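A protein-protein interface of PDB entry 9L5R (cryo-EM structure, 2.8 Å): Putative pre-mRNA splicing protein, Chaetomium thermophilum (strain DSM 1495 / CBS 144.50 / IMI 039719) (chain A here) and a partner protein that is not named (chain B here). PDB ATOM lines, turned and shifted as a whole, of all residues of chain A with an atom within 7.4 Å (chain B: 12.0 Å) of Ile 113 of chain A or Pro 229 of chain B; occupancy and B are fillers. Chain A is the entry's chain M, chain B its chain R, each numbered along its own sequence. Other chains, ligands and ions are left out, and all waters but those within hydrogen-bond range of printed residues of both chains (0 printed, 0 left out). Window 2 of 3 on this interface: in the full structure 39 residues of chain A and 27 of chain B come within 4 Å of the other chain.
O of Pro 229 of chain B is in hydrogen-bond range of NE2 of Gln 120 of chain A (2.8 Å).
The side-chain amino group (NZ) of Lys 226 of chain B is in salt-bridge range of the side-chain carboxylate (OE2) of Glu 116 of chain A, at 3.0 Å.
Of the 10 printed residues of chain B, 6 touch a printed residue of chain A.
Among the printed residues, 14 pairs touch across the chains.
Among the printed residues, Asp or Glu carboxylates within 4 Å of a Lys or Arg side-chain nitrogen of the other chain: Glu 116 of chain A with Lys 226 of chain B (3.0 Å).
The side-chain amide nitrogen of Gln 120 of chain A sits close to the side-chain amide oxygen of Asn 121 of chain A.
ND2 of Asn 121 of chain A lies close to O of Tyr 117 of chain A (3.2 Å).
The backbone carbonyl oxygen (O) of Glu 112 of chain A sits close to the side-chain carboxylate (OE1) of Glu 116 of chain A, 2.6 Å away.
Ile 113 of chain A touches just one residue of chain B: Pro 229 (3.8 Å).
No residue of chain B comes within 4 Å of Ser 111 of chain A.
No residue of chain B comes within 4 Å of Glu 112 of chain A.
No residue of chain B comes within 4 Å of Asn 114 of chain A.
No residue of chain B comes within 4 Å of Arg 115 of chain A.
Tyr 117 of chain A touches just these residues of chain B: Ile 228, Pro 229, Arg 230, Gly 231 and Pro 232.
Of the printed residues of chain A, Arg 230 of chain B touches Tyr 117 and Gln 120.
Of the printed residues of chain B, Asn 121 of chain A touches Gly 231 (3.2 Å) and Pro 232 (3.5 Å).
Of the printed residues of chain B, Gln 120 of chain A touches Ile 228 (3.9 Å), Pro 229 (2.8 Å), Arg 230 (3.98 Å) and Gly 231 (3.5 Å).
Of the printed residues of chain A, Gly 231 of chain B touches Tyr 117, Gln 120 and Asn 121.
Pro 233 of chain B touches none of the printed residues of chain A.
Gln 110 of chain A touches none of the printed residues of chain B.
The nearest residue of chain A that does not touch Pro 229 of chain B is Asn 121 of chain A (5.4 Å).
The nearest printed residue of chain A that does not touch Lys 226 of chain B is Arg 115 of chain A (6.0 Å).
Ile 113 of chain A touches Pro 229 of chain B.
CA of Tyr 117 of chain A touches CG2 of Ile 228 of chain B, 3.8 Å away.
Tyr 117 of chain A touches Pro 229 of chain B (CD1 to O, 3.4 Å).
Tyr 117 of chain A touches Arg 230 of chain B (CE1 to O, 3.6 Å).
Gly 231 of chain B touches Tyr 117 of chain A (CA to CE1, 3.8 Å).
CD of Pro 232 of chain B touches OH of Tyr 117 of chain A, at 3.3 Å.
Gln 120 of chain A touches Ile 228 of chain B.
Gln 120 of chain A touches Arg 230 of chain B.
OD1 of Asn 121 of chain A touches CA of Gly 231 of chain B, at 3.2 Å.
CD of Pro 232 of chain B touches ND2 of Asn 121 of chain A, at 3.5 Å.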
ATOM      1  N   GLN A 110      33.591 -19.551  13.269  1.00  0.00           N
ATOM      2  CA  GLN A 110      33.318 -20.909  12.835  1.00  0.00           C
ATOM      3  C   GLN A 110      31.830 -21.226  12.685  1.00  0.00           C
ATOM      4  O   GLN A 110      31.492 -22.256  12.091  1.00  0.00           O
ATOM      5  CB  GLN A 110      34.025 -21.893  13.787  1.00  0.00           C
ATOM      6  CG  GLN A 110      33.971 -23.356  13.416  1.00  0.00           C
ATOM      7  CD  GLN A 110      34.658 -23.652  12.098  1.00  0.00           C
ATOM      8  OE1 GLN A 110      35.723 -23.119  11.795  1.00  0.00           O
ATOM      9  NE2 GLN A 110      34.035 -24.504  11.295  1.00  0.00           N
ATOM     10  N   SER A 111      30.937 -20.339  13.111  1.00  0.00           N
ATOM     11  CA  SER A 111      29.543 -20.430  12.704  1.00  0.00           C
ATOM     12  C   SER A 111      29.438 -20.389  11.182  1.00  0.00           C
ATOM     13  O   SER A 111      30.317 -19.874  10.491  1.00  0.00           O
ATOM     14  CB  SER A 111      28.734 -19.292  13.310  1.00  0.00           C
ATOM     15  OG  SER A 111      27.355 -19.588  13.287  1.00  0.00           O
ATOM     16  N   GLU A 112      28.335 -20.929  10.671  1.00  0.00           N
ATOM     17  CA  GLU A 112      28.245 -21.359   9.282  1.00  0.00           C
ATOM     18  C   GLU A 112      28.475 -20.243   8.269  1.00  0.00           C
ATOM     19  O   GLU A 112      29.585 -20.093   7.725  1.00  0.00           O
ATOM     20  CB  GLU A 112      26.867 -21.971   9.061  1.00  0.00           C
ATOM     21  CG  GLU A 112      26.480 -22.930  10.161  1.00  0.00           C
ATOM     22  CD  GLU A 112      27.347 -24.167  10.192  1.00  0.00           C
ATOM     23  OE1 GLU A 112      27.697 -24.668   9.105  1.00  0.00           O
ATOM     24  OE2 GLU A 112      27.682 -24.629  11.301  1.00  0.00           O
ATOM     25  N   ILE A 113      27.499 -19.351   8.107  1.00  0.00           N
ATOM     26  CA  ILE A 113      27.707 -18.379   7.046  1.00  0.00           C
ATOM     27  C   ILE A 113      28.629 -17.268   7.508  1.00  0.00           C
ATOM     28  O   ILE A 113      29.175 -16.554   6.665  1.00  0.00           O
ATOM     29  CB  ILE A 113      26.430 -17.743   6.483  1.00  0.00           C
ATOM     30  CG1 ILE A 113      25.882 -16.723   7.432  1.00  0.00           C
ATOM     31  CG2 ILE A 113      25.361 -18.797   6.314  1.00  0.00           C
ATOM     32  CD1 ILE A 113      25.031 -15.794   6.723  1.00  0.00           C
ATOM     33  N   ASN A 114      28.865 -17.159   8.818  1.00  0.00           N
ATOM     34  CA  ASN A 114      29.900 -16.268   9.321  1.00  0.00           C
ATOM     35  C   ASN A 114      31.266 -16.659   8.793  1.00  0.00           C
ATOM     36  O   ASN A 114      32.054 -15.792   8.407  1.00  0.00           O
ATOM     37  CB  ASN A 114      29.923 -16.275  10.846  1.00  0.00           C
ATOM     38  CG  ASN A 114      28.799 -15.492  11.448  1.00  0.00           C
ATOM     39  OD1 ASN A 114      28.450 -14.419  10.974  1.00  0.00           O
ATOM     40  ND2 ASN A 114      28.218 -16.023  12.507  1.00  0.00           N
ATOM     41  N   ARG A 115      31.566 -17.959   8.750  1.00  0.00           N
ATOM     42  CA  ARG A 115      32.893 -18.351   8.308  1.00  0.00           C
ATOM     43  C   ARG A 115      33.029 -18.223   6.799  1.00  0.00           C
ATOM     44  O   ARG A 115      34.095 -17.796   6.328  1.00  0.00           O
ATOM     45  CB  ARG A 115      33.256 -19.764   8.790  1.00  0.00           C
ATOM     46  CG  ARG A 115      32.489 -20.871   8.147  1.00  0.00           C
ATOM     47  CD  ARG A 115      32.932 -22.244   8.448  1.00  0.00           C
ATOM     48  NE  ARG A 115      31.953 -23.149   7.864  1.00  0.00           N
ATOM     49  CZ  ARG A 115      31.123 -23.900   8.570  1.00  0.00           C
ATOM     50  NH1 ARG A 115      31.191 -23.950   9.888  1.00  0.00           N
ATOM     51  NH2 ARG A 115      30.194 -24.607   7.938  1.00  0.00           N
ATOM     52  N   GLU A 116      31.968 -18.531   6.006  1.00  0.00           N
ATOM     53  CA  GLU A 116      32.168 -18.241   4.575  1.00  0.00           C
ATOM     54  C   GLU A 116      32.270 -16.737   4.315  1.00  0.00           C
ATOM     55  O   GLU A 116      33.045 -16.311   3.453  1.00  0.00           O
ATOM     56  CB  GLU A 116      31.115 -18.788   3.595  1.00  0.00           C
ATOM     57  CG  GLU A 116      30.937 -20.294   3.360  1.00  0.00           C
ATOM     58  CD  GLU A 116      30.039 -20.926   4.359  1.00  0.00           C
ATOM     59  OE1 GLU A 116      29.524 -20.155   5.141  1.00  0.00           O
ATOM     60  OE2 GLU A 116      29.846 -22.156   4.380  1.00  0.00           O
ATOM     61  N   TYR A 117      31.490 -15.925   5.037  1.00  0.00           N
ATOM     62  CA  TYR A 117      31.496 -14.473   4.850  1.00  0.00           C
ATOM     63  C   TYR A 117      32.843 -13.871   5.194  1.00  0.00           C
ATOM     64  O   TYR A 117      33.371 -13.036   4.452  1.00  0.00           O
ATOM     65  CB  TYR A 117      30.398 -13.876   5.721  1.00  0.00           C
ATOM     66  CG  TYR A 117      30.227 -12.386   5.732  1.00  0.00           C
ATOM     67  CD1 TYR A 117      29.472 -11.749   4.756  1.00  0.00           C
ATOM     68  CD2 TYR A 117      30.749 -11.624   6.760  1.00  0.00           C
ATOM     69  CE1 TYR A 117      29.285 -10.399   4.786  1.00  0.00           C
ATOM     70  CE2 TYR A 117      30.563 -10.276   6.799  1.00  0.00           C
ATOM     71  CZ  TYR A 117      29.829  -9.668   5.817  1.00  0.00           C
ATOM     72  OH  TYR A 117      29.650  -8.324   5.859  1.00  0.00           O
ATOM     73  N   PHE A 118      33.424 -14.314   6.307  1.00  0.00           N
ATOM     74  CA  PHE A 118      34.742 -13.867   6.719  1.00  0.00           C
ATOM     75  C   PHE A 118      35.804 -14.259   5.702  1.00  0.00           C
ATOM     76  O   PHE A 118      36.661 -13.443   5.341  1.00  0.00           O
ATOM     77  CB  PHE A 118      35.047 -14.452   8.093  1.00  0.00           C
ATOM     78  CG  PHE A 118      36.349 -14.018   8.675  1.00  0.00           C
ATOM     79  CD1 PHE A 118      36.477 -12.784   9.271  1.00  0.00           C
ATOM     80  CD2 PHE A 118      37.443 -14.860   8.652  1.00  0.00           C
ATOM     81  CE1 PHE A 118      37.671 -12.390   9.816  1.00  0.00           C
ATOM     82  CE2 PHE A 118      38.642 -14.472   9.203  1.00  0.00           C
ATOM     83  CZ  PHE A 118      38.754 -13.232   9.788  1.00  0.00           C
ATOM     84  N   ALA A 119      35.760 -15.500   5.214  1.00  0.00           N
ATOM     85  CA  ALA A 119      36.764 -15.929   4.244  1.00  0.00           C
ATOM     86  C   ALA A 119      36.635 -15.184   2.920  1.00  0.00           C
ATOM     87  O   ALA A 119      37.646 -14.787   2.335  1.00  0.00           O
ATOM     88  CB  ALA A 119      36.675 -17.431   4.023  1.00  0.00           C
ATOM     89  N   GLN A 120      35.406 -14.961   2.442  1.00  0.00           N
ATOM     90  CA  GLN A 120      35.230 -14.236   1.189  1.00  0.00           C
ATOM     91  C   GLN A 120      35.673 -12.781   1.320  1.00  0.00           C
ATOM     92  O   GLN A 120      36.287 -12.236   0.397  1.00  0.00           O
ATOM     93  CB  GLN A 120      33.780 -14.343   0.705  1.00  0.00           C
ATOM     94  CG  GLN A 120      32.838 -13.353   1.309  1.00  0.00           C
ATOM     95  CD  GLN A 120      31.579 -13.114   0.552  1.00  0.00           C
ATOM     96  OE1 GLN A 120      31.322 -13.735  -0.468  1.00  0.00           O
ATOM     97  NE2 GLN A 120      30.761 -12.204   1.069  1.00  0.00           N
ATOM     98  N   ASN A 121      35.453 -12.156   2.482  1.00  0.00           N
ATOM     99  CA  ASN A 121      35.840 -10.763   2.618  1.00  0.00           C
ATOM    100  C   ASN A 121      37.348 -10.626   2.746  1.00  0.00           C
ATOM    101  O   ASN A 121      37.943  -9.725   2.147  1.00  0.00           O
ATOM    102  CB  ASN A 121      35.113 -10.139   3.801  1.00  0.00           C
ATOM    103  CG  ASN A 121      33.619 -10.087   3.589  1.00  0.00           C
ATOM    104  OD1 ASN A 121      33.145 -10.215   2.475  1.00  0.00           O
ATOM    105  ND2 ASN A 121      32.874  -9.929   4.655  1.00  0.00           N
ATOM    106  N   LYS B 224      27.515 -28.261  -3.758  1.00  0.00           N
ATOM    107  CA  LYS B 224      26.346 -27.411  -3.841  1.00  0.00           C
ATOM    108  C   LYS B 224      26.723 -25.971  -3.524  1.00  0.00           C
ATOM    109  O   LYS B 224      27.517 -25.705  -2.623  1.00  0.00           O
ATOM    110  CB  LYS B 224      25.276 -27.922  -2.887  1.00  0.00           C
ATOM    111  CG  LYS B 224      23.982 -27.191  -2.951  1.00  0.00           C
ATOM    112  CD  LYS B 224      22.964 -27.801  -2.024  1.00  0.00           C
ATOM    113  CE  LYS B 224      21.676 -26.997  -2.041  1.00  0.00           C
ATOM    114  NZ  LYS B 224      20.673 -27.555  -1.113  1.00  0.00           N
ATOM    115  N   HIS B 225      26.171 -25.039  -4.283  1.00  0.00           N
ATOM    116  CA  HIS B 225      26.497 -23.635  -4.096  1.00  0.00           C
ATOM    117  C   HIS B 225      25.748 -23.067  -2.895  1.00  0.00           C
ATOM    118  O   HIS B 225      24.765 -23.634  -2.418  1.00  0.00           O
ATOM    119  CB  HIS B 225      26.174 -22.840  -5.351  1.00  0.00           C
ATOM    120  CG  HIS B 225      26.953 -23.269  -6.550  1.00  0.00           C
ATOM    121  ND1 HIS B 225      26.651 -22.853  -7.826  1.00  0.00           N
ATOM    122  CD2 HIS B 225      28.026 -24.081  -6.666  1.00  0.00           C
ATOM    123  CE1 HIS B 225      27.502 -23.391  -8.677  1.00  0.00           C
ATOM    124  NE2 HIS B 225      28.345 -24.144  -7.998  1.00  0.00           N
ATOM    125  N   LYS B 226      26.243 -21.941  -2.389  1.00  0.00           N
ATOM    126  CA  LYS B 226      25.716 -21.346  -1.170  1.00  0.00           C
ATOM    127  C   LYS B 226      25.446 -19.863  -1.368  1.00  0.00           C
ATOM    128  O   LYS B 226      26.080 -19.207  -2.191  1.00  0.00           O
ATOM    129  CB  LYS B 226      26.676 -21.549  -0.003  1.00  0.00           C
ATOM    130  CG  LYS B 226      26.764 -22.988   0.466  1.00  0.00           C
ATOM    131  CD  LYS B 226      27.790 -23.173   1.554  1.00  0.00           C
ATOM    132  CE  LYS B 226      29.183 -23.251   0.977  1.00  0.00           C
ATOM    133  NZ  LYS B 226      30.152 -23.803   1.949  1.00  0.00           N
ATOM    134  N   LYS B 227      24.481 -19.352  -0.611  1.00  0.00           N
ATOM    135  CA  LYS B 227      24.141 -17.933  -0.577  1.00  0.00           C
ATOM    136  C   LYS B 227      24.860 -17.313   0.608  1.00  0.00           C
ATOM    137  O   LYS B 227      24.603 -17.676   1.756  1.00  0.00           O
ATOM    138  CB  LYS B 227      22.634 -17.710  -0.440  1.00  0.00           C
ATOM    139  CG  LYS B 227      21.789 -18.268  -1.552  1.00  0.00           C
ATOM    140  CD  LYS B 227      20.460 -17.538  -1.667  1.00  0.00           C
ATOM    141  CE  LYS B 227      19.564 -17.809  -0.492  1.00  0.00           C
ATOM    142  NZ  LYS B 227      18.163 -17.563  -0.848  1.00  0.00           N
ATOM    143  N   ILE B 228      25.765 -16.392   0.326  1.00  0.00           N
ATOM    144  CA  ILE B 228      26.505 -15.658   1.343  1.00  0.00           C
ATOM    145  C   ILE B 228      26.144 -14.202   1.106  1.00  0.00           C
ATOM    146  O   ILE B 228      26.092 -13.774  -0.051  1.00  0.00           O
ATOM    147  CB  ILE B 228      28.021 -15.914   1.232  1.00  0.00           C
ATOM    148  CG1 ILE B 228      28.310 -17.412   1.128  1.00  0.00           C
ATOM    149  CG2 ILE B 228      28.771 -15.339   2.407  1.00  0.00           C
ATOM    150  CD1 ILE B 228      27.795 -18.230   2.299  1.00  0.00           C
ATOM    151  N   PRO B 229      25.845 -13.424   2.139  1.00  0.00           N
ATOM    152  CA  PRO B 229      25.638 -11.991   1.931  1.00  0.00           C
ATOM    153  C   PRO B 229      26.899 -11.350   1.387  1.00  0.00           C
ATOM    154  O   PRO B 229      28.010 -11.794   1.674  1.00  0.00           O
ATOM    155  CB  PRO B 229      25.292 -11.470   3.326  1.00  0.00           C
ATOM    156  CG  PRO B 229      25.571 -12.557   4.240  1.00  0.00           C
ATOM    157  CD  PRO B 229      25.554 -13.827   3.519  1.00  0.00           C
ATOM    158  N   ARG B 230      26.715 -10.355   0.528  1.00  0.00           N
ATOM    159  CA  ARG B 230      27.859  -9.640  -0.015  1.00  0.00           C
ATOM    160  C   ARG B 230      28.567  -8.889   1.101  1.00  0.00           C
ATOM    161  O   ARG B 230      27.949  -8.428   2.064  1.00  0.00           O
ATOM    162  CB  ARG B 230      27.430  -8.679  -1.125  1.00  0.00           C
ATOM    163  CG  ARG B 230      26.530  -7.565  -0.652  1.00  0.00           C
ATOM    164  CD  ARG B 230      26.459  -6.443  -1.642  1.00  0.00           C
ATOM    165  NE  ARG B 230      25.488  -6.719  -2.685  1.00  0.00           N
ATOM    166  CZ  ARG B 230      25.685  -6.476  -3.970  1.00  0.00           C
ATOM    167  NH1 ARG B 230      26.804  -5.925  -4.402  1.00  0.00           N
ATOM    168  NH2 ARG B 230      24.734  -6.795  -4.842  1.00  0.00           N
ATOM    169  N   GLY B 231      29.882  -8.794   0.972  1.00  0.00           N
ATOM    170  CA  GLY B 231      30.699  -8.183   1.982  1.00  0.00           C
ATOM    171  C   GLY B 231      30.573  -6.679   1.984  1.00  0.00           C
ATOM    172  O   GLY B 231      29.952  -6.081   1.102  1.00  0.00           O
ATOM    173  N   PRO B 232      31.143  -6.045   3.001  1.00  0.00           N
ATOM    174  CA  PRO B 232      31.077  -4.600   3.116  1.00  0.00           C
ATOM    175  C   PRO B 232      31.849  -3.924   2.002  1.00  0.00           C
ATOM    176  O   PRO B 232      32.786  -4.512   1.443  1.00  0.00           O
ATOM    177  CB  PRO B 232      31.730  -4.332   4.476  1.00  0.00           C
ATOM    178  CG  PRO B 232      32.541  -5.482   4.733  1.00  0.00           C
ATOM    179  CD  PRO B 232      31.846  -6.641   4.141  1.00  0.00           C
ATOM    180  N   PRO B 233      31.496  -2.683   1.651  1.00  0.00           N
ATOM    181  CA  PRO B 233      32.282  -1.975   0.641  1.00  0.00           C
ATOM    182  C   PRO B 233      33.719  -1.671   1.082  1.00  0.00           C
ATOM    183  O   PRO B 233      34.125  -1.958   2.197  1.00  0.00           O
ATOM    184  CB  PRO B 233      31.507  -0.681   0.443  1.00  0.00           C
ATOM    185  CG  PRO B 233      30.755  -0.487   1.677  1.00  0.00           C
ATOM    186  CD  PRO B 233      30.421  -1.839   2.200  1.00  0.00           C
